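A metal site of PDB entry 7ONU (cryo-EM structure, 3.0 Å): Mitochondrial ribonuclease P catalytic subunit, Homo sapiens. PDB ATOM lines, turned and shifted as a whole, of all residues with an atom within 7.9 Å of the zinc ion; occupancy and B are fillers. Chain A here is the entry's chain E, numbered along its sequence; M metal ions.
His 538 touches the zinc ion (CE1 to ZN, 3.5 Å). Five residues have an atom within 4 Å of the zinc ion: Cys 306, Cys 309, His 515, Cys 536 and His 538. The nearest printed residue that does not touch the zinc ion is Lys 311 (4.6 Å).
The zinc ion is bound by NE2 of His 515 (2.1 Å), SG of Cys 309 (2.3 Å), SG of Cys 306 (2.3 Å) and SG of Cys 536 (2.3 Å). The zinc ion has four donor atoms within binding distance.
OG of Ser 513 lies close to ND1 of His 515 (3.4 Å). SG of Cys 309 sits close to NE2 of His 538. The side-chain sulfur (SG) of Cys 309 lies close to the backbone NH (N) of Lys 311 (3.5 Å). The backbone carbonyl oxygen (O) of Lys 311 sits at hydrogen-bond distance from the backbone NH (N) of Cys 306, 3.3 Å away. NE2 of His 538 lies close to SG of Cys 536. O of Cys 536 is in hydrogen-bond range of N of Gln 296 (2.9 Å).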
ATOM      1  N   GLN A 296      22.029 -18.186  -1.142  1.00  0.00           N
ATOM      2  CA  GLN A 296      22.095 -17.861   0.272  1.00  0.00           C
ATOM      3  C   GLN A 296      20.852 -17.066   0.650  1.00  0.00           C
ATOM      4  O   GLN A 296      20.259 -16.384  -0.189  1.00  0.00           O
ATOM      5  CB  GLN A 296      23.351 -17.047   0.599  1.00  0.00           C
ATOM      6  CG  GLN A 296      24.636 -17.815   0.431  1.00  0.00           C
ATOM      7  CD  GLN A 296      25.856 -16.938   0.627  1.00  0.00           C
ATOM      8  OE1 GLN A 296      25.739 -15.729   0.763  1.00  0.00           O
ATOM      9  NE2 GLN A 296      27.030 -17.557   0.626  1.00  0.00           N
ATOM     10  N   THR A 298      19.912 -14.037   2.851  1.00  0.00           N
ATOM     11  CA  THR A 298      20.634 -12.922   3.446  1.00  0.00           C
ATOM     12  C   THR A 298      19.704 -11.758   3.745  1.00  0.00           C
ATOM     13  O   THR A 298      18.476 -11.890   3.659  1.00  0.00           O
ATOM     14  CB  THR A 298      21.754 -12.461   2.514  1.00  0.00           C
ATOM     15  OG1 THR A 298      21.178 -11.915   1.319  1.00  0.00           O
ATOM     16  CG2 THR A 298      22.653 -13.619   2.142  1.00  0.00           C
ATOM     17  N   THR A 299      20.274 -10.618   4.106  1.00  0.00           N
ATOM     18  CA  THR A 299      19.542  -9.385   4.309  1.00  0.00           C
ATOM     19  C   THR A 299      20.383  -8.242   3.750  1.00  0.00           C
ATOM     20  O   THR A 299      21.582  -8.389   3.510  1.00  0.00           O
ATOM     21  CB  THR A 299      19.198  -9.156   5.779  1.00  0.00           C
ATOM     22  OG1 THR A 299      18.259  -8.068   5.891  1.00  0.00           O
ATOM     23  CG2 THR A 299      20.446  -8.814   6.574  1.00  0.00           C
ATOM     24  N   VAL A 300      19.740  -7.088   3.547  1.00  0.00           N
ATOM     25  CA  VAL A 300      20.380  -5.950   2.920  1.00  0.00           C
ATOM     26  C   VAL A 300      20.736  -4.926   3.994  1.00  0.00           C
ATOM     27  O   VAL A 300      19.890  -4.552   4.808  1.00  0.00           O
ATOM     28  CB  VAL A 300      19.491  -5.323   1.832  1.00  0.00           C
ATOM     29  CG1 VAL A 300      19.990  -3.942   1.450  1.00  0.00           C
ATOM     30  CG2 VAL A 300      19.462  -6.217   0.610  1.00  0.00           C
ATOM     31  N   GLN A 305      23.534  -2.750   0.630  1.00  0.00           N
ATOM     32  CA  GLN A 305      24.441  -3.823   0.243  1.00  0.00           C
ATOM     33  C   GLN A 305      24.047  -5.091   0.997  1.00  0.00           C
ATOM     34  O   GLN A 305      23.978  -5.070   2.230  1.00  0.00           O
ATOM     35  CB  GLN A 305      25.888  -3.450   0.548  1.00  0.00           C
ATOM     36  CG  GLN A 305      26.414  -2.299  -0.289  1.00  0.00           C
ATOM     37  CD  GLN A 305      27.776  -1.828   0.177  1.00  0.00           C
ATOM     38  OE1 GLN A 305      27.890  -0.804   0.850  1.00  0.00           O
ATOM     39  NE2 GLN A 305      28.812  -2.578  -0.169  1.00  0.00           N
ATOM     40  N   CYS A 306      23.801  -6.177   0.271  1.00  0.00           N
ATOM     41  CA  CYS A 306      23.373  -7.398   0.938  1.00  0.00           C
ATOM     42  C   CYS A 306      24.562  -8.082   1.590  1.00  0.00           C
ATOM     43  O   CYS A 306      25.694  -7.990   1.117  1.00  0.00           O
ATOM     44  CB  CYS A 306      22.677  -8.360  -0.033  1.00  0.00           C
ATOM     45  SG  CYS A 306      23.679  -9.031  -1.368  1.00  0.00           S
ATOM     46  N   SER A 307      24.292  -8.759   2.703  1.00  0.00           N
ATOM     47  CA  SER A 307      25.359  -9.345   3.496  1.00  0.00           C
ATOM     48  C   SER A 307      26.045 -10.487   2.769  1.00  0.00           C
ATOM     49  O   SER A 307      27.221 -10.757   3.012  1.00  0.00           O
ATOM     50  CB  SER A 307      24.794  -9.828   4.829  1.00  0.00           C
ATOM     51  OG  SER A 307      24.156  -8.781   5.520  1.00  0.00           O
ATOM     52  N   GLY A 308      25.333 -11.167   1.862  1.00  0.00           N
ATOM     53  CA  GLY A 308      25.891 -12.353   1.244  1.00  0.00           C
ATOM     54  C   GLY A 308      27.157 -12.090   0.460  1.00  0.00           C
ATOM     55  O   GLY A 308      28.090 -12.899   0.476  1.00  0.00           O
ATOM     56  N   CYS A 309      27.214 -10.960  -0.248  1.00  0.00           N
ATOM     57  CA  CYS A 309      28.368 -10.636  -1.078  1.00  0.00           C
ATOM     58  C   CYS A 309      28.830  -9.191  -0.989  1.00  0.00           C
ATOM     59  O   CYS A 309      29.951  -8.895  -1.416  1.00  0.00           O
ATOM     60  CB  CYS A 309      28.071 -10.935  -2.548  1.00  0.00           C
ATOM     61  SG  CYS A 309      26.656 -10.043  -3.182  1.00  0.00           S
ATOM     62  N   GLY A 310      28.016  -8.271  -0.467  1.00  0.00           N
ATOM     63  CA  GLY A 310      28.381  -6.873  -0.414  1.00  0.00           C
ATOM     64  C   GLY A 310      28.007  -6.059  -1.628  1.00  0.00           C
ATOM     65  O   GLY A 310      28.155  -4.827  -1.586  1.00  0.00           O
ATOM     66  N   LYS A 311      27.519  -6.684  -2.689  1.00  0.00           N
ATOM     67  CA  LYS A 311      27.087  -5.930  -3.863  1.00  0.00           C
ATOM     68  C   LYS A 311      25.934  -5.017  -3.509  1.00  0.00           C
ATOM     69  O   LYS A 311      25.156  -5.293  -2.585  1.00  0.00           O
ATOM     70  CB  LYS A 311      26.689  -6.876  -4.990  1.00  0.00           C
ATOM     71  CG  LYS A 311      27.839  -7.663  -5.577  1.00  0.00           C
ATOM     72  CD  LYS A 311      27.362  -8.667  -6.624  1.00  0.00           C
ATOM     73  CE  LYS A 311      26.686  -7.981  -7.795  1.00  0.00           C
ATOM     74  NZ  LYS A 311      27.531  -6.906  -8.387  1.00  0.00           N
ATOM     75  N   THR A 312      25.814  -3.917  -4.247  1.00  0.00           N
ATOM     76  CA  THR A 312      24.801  -2.904  -3.966  1.00  0.00           C
ATOM     77  C   THR A 312      23.499  -3.241  -4.679  1.00  0.00           C
ATOM     78  O   THR A 312      23.503  -3.538  -5.884  1.00  0.00           O
ATOM     79  CB  THR A 312      25.284  -1.524  -4.400  1.00  0.00           C
ATOM     80  OG1 THR A 312      25.675  -1.558  -5.769  1.00  0.00           O
ATOM     81  CG2 THR A 312      26.455  -1.069  -3.552  1.00  0.00           C
ATOM     82  N   ILE A 313      22.389  -3.204  -3.941  1.00  0.00           N
ATOM     83  CA  ILE A 313      21.063  -3.405  -4.505  1.00  0.00           C
ATOM     84  C   ILE A 313      20.762  -2.237  -5.425  1.00  0.00           C
ATOM     85  O   ILE A 313      21.448  -1.216  -5.385  1.00  0.00           O
ATOM     86  CB  ILE A 313      20.014  -3.543  -3.386  1.00  0.00           C
ATOM     87  CG1 ILE A 313      20.419  -4.629  -2.387  1.00  0.00           C
ATOM     88  CG2 ILE A 313      18.646  -3.874  -3.953  1.00  0.00           C
ATOM     89  CD1 ILE A 313      20.808  -5.943  -3.018  1.00  0.00           C
ATOM     90  N   SER A 513      24.379 -12.345 -11.367  1.00  0.00           N
ATOM     91  CA  SER A 513      23.807 -12.376 -10.026  1.00  0.00           C
ATOM     92  C   SER A 513      22.297 -12.184 -10.064  1.00  0.00           C
ATOM     93  O   SER A 513      21.765 -11.461 -10.906  1.00  0.00           O
ATOM     94  CB  SER A 513      24.442 -11.308  -9.157  1.00  0.00           C
ATOM     95  OG  SER A 513      23.918 -11.335  -7.840  1.00  0.00           O
ATOM     96  N   TRP A 514      21.607 -12.824  -9.121  1.00  0.00           N
ATOM     97  CA  TRP A 514      20.159 -12.711  -8.961  1.00  0.00           C
ATOM     98  C   TRP A 514      19.859 -12.401  -7.504  1.00  0.00           C
ATOM     99  O   TRP A 514      20.294 -13.131  -6.607  1.00  0.00           O
ATOM    100  CB  TRP A 514      19.456 -14.002  -9.350  1.00  0.00           C
ATOM    101  CG  TRP A 514      18.984 -14.087 -10.773  1.00  0.00           C
ATOM    102  CD1 TRP A 514      19.580 -14.764 -11.786  1.00  0.00           C
ATOM    103  CD2 TRP A 514      17.805 -13.490 -11.317  1.00  0.00           C
ATOM    104  NE1 TRP A 514      18.847 -14.616 -12.939  1.00  0.00           N
ATOM    105  CE2 TRP A 514      17.757 -13.844 -12.681  1.00  0.00           C
ATOM    106  CE3 TRP A 514      16.786 -12.688 -10.788  1.00  0.00           C
ATOM    107  CZ2 TRP A 514      16.728 -13.430 -13.519  1.00  0.00           C
ATOM    108  CZ3 TRP A 514      15.771 -12.273 -11.627  1.00  0.00           C
ATOM    109  CH2 TRP A 514      15.746 -12.643 -12.977  1.00  0.00           C
ATOM    110  N   HIS A 515      19.111 -11.331  -7.245  1.00  0.00           N
ATOM    111  CA  HIS A 515      18.670 -10.996  -5.897  1.00  0.00           C
ATOM    112  C   HIS A 515      17.153 -10.986  -5.872  1.00  0.00           C
ATOM    113  O   HIS A 515      16.525 -10.285  -6.664  1.00  0.00           O
ATOM    114  CB  HIS A 515      19.229  -9.644  -5.460  1.00  0.00           C
ATOM    115  CG  HIS A 515      20.654  -9.701  -5.002  1.00  0.00           C
ATOM    116  ND1 HIS A 515      21.712  -9.678  -5.880  1.00  0.00           N
ATOM    117  CD2 HIS A 515      21.193  -9.773  -3.764  1.00  0.00           C
ATOM    118  CE1 HIS A 515      22.840  -9.732  -5.199  1.00  0.00           C
ATOM    119  NE2 HIS A 515      22.551  -9.802  -3.915  1.00  0.00           N
ATOM    120  N   TRP A 534      16.182 -11.752   1.872  1.00  0.00           N
ATOM    121  CA  TRP A 534      16.593 -11.768   0.486  1.00  0.00           C
ATOM    122  C   TRP A 534      17.180 -13.129   0.156  1.00  0.00           C
ATOM    123  O   TRP A 534      17.677 -13.837   1.035  1.00  0.00           O
ATOM    124  CB  TRP A 534      17.624 -10.679   0.178  1.00  0.00           C
ATOM    125  CG  TRP A 534      17.062  -9.295   0.064  1.00  0.00           C
ATOM    126  CD1 TRP A 534      16.637  -8.504   1.094  1.00  0.00           C
ATOM    127  CD2 TRP A 534      16.884  -8.540  -1.125  1.00  0.00           C
ATOM    128  NE1 TRP A 534      16.207  -7.298   0.602  1.00  0.00           N
ATOM    129  CE2 TRP A 534      16.341  -7.290  -0.754  1.00  0.00           C
ATOM    130  CE3 TRP A 534      17.126  -8.782  -2.485  1.00  0.00           C
ATOM    131  CZ2 TRP A 534      16.037  -6.302  -1.686  1.00  0.00           C
ATOM    132  CZ3 TRP A 534      16.824  -7.803  -3.394  1.00  0.00           C
ATOM    133  CH2 TRP A 534      16.291  -6.580  -2.994  1.00  0.00           C
ATOM    134  N   LEU A 535      17.150 -13.484  -1.115  1.00  0.00           N
ATOM    135  CA  LEU A 535      17.804 -14.674  -1.640  1.00  0.00           C
ATOM    136  C   LEU A 535      18.821 -14.217  -2.663  1.00  0.00           C
ATOM    137  O   LEU A 535      18.461 -13.602  -3.674  1.00  0.00           O
ATOM    138  CB  LEU A 535      16.779 -15.625  -2.277  1.00  0.00           C
ATOM    139  CG  LEU A 535      17.344 -16.856  -2.976  1.00  0.00           C
ATOM    140  CD1 LEU A 535      17.649 -17.935  -1.977  1.00  0.00           C
ATOM    141  CD2 LEU A 535      16.381 -17.352  -4.024  1.00  0.00           C
ATOM    142  N   CYS A 536      20.098 -14.504  -2.406  1.00  0.00           N
ATOM    143  CA  CYS A 536      21.193 -14.047  -3.243  1.00  0.00           C
ATOM    144  C   CYS A 536      21.778 -15.260  -3.958  1.00  0.00           C
ATOM    145  O   CYS A 536      22.142 -16.249  -3.308  1.00  0.00           O
ATOM    146  CB  CYS A 536      22.242 -13.341  -2.381  1.00  0.00           C
ATOM    147  SG  CYS A 536      23.635 -12.563  -3.231  1.00  0.00           S
ATOM    148  N   LEU A 537      21.852 -15.190  -5.290  1.00  0.00           N
ATOM    149  CA  LEU A 537      22.312 -16.298  -6.126  1.00  0.00           C
ATOM    150  C   LEU A 537      23.430 -15.802  -7.036  1.00  0.00           C
ATOM    151  O   LEU A 537      23.220 -14.865  -7.809  1.00  0.00           O
ATOM    152  CB  LEU A 537      21.169 -16.861  -6.974  1.00  0.00           C
ATOM    153  CG  LEU A 537      19.894 -17.386  -6.303  1.00  0.00           C
ATOM    154  CD1 LEU A 537      18.771 -17.462  -7.311  1.00  0.00           C
ATOM    155  CD2 LEU A 537      20.140 -18.754  -5.709  1.00  0.00           C
ATOM    156  N   HIS A 538      24.595 -16.440  -6.948  1.00  0.00           N
ATOM    157  CA  HIS A 538      25.754 -16.058  -7.754  1.00  0.00           C
ATOM    158  C   HIS A 538      26.199 -17.198  -8.644  1.00  0.00           C
ATOM    159  O   HIS A 538      26.340 -18.335  -8.197  1.00  0.00           O
ATOM    160  CB  HIS A 538      26.913 -15.624  -6.869  1.00  0.00           C
ATOM    161  CG  HIS A 538      26.536 -14.594  -5.866  1.00  0.00           C
ATOM    162  ND1 HIS A 538      26.745 -13.248  -6.087  1.00  0.00           N
ATOM    163  CD2 HIS A 538      25.970 -14.695  -4.642  1.00  0.00           C
ATOM    164  CE1 HIS A 538      26.314 -12.570  -5.035  1.00  0.00           C
ATOM    165  NE2 HIS A 538      25.841 -13.423  -4.149  1.00  0.00           N
HETATM  166 ZN    ZN M   1      24.367 -10.351  -3.136  1.00  0.00          ZN
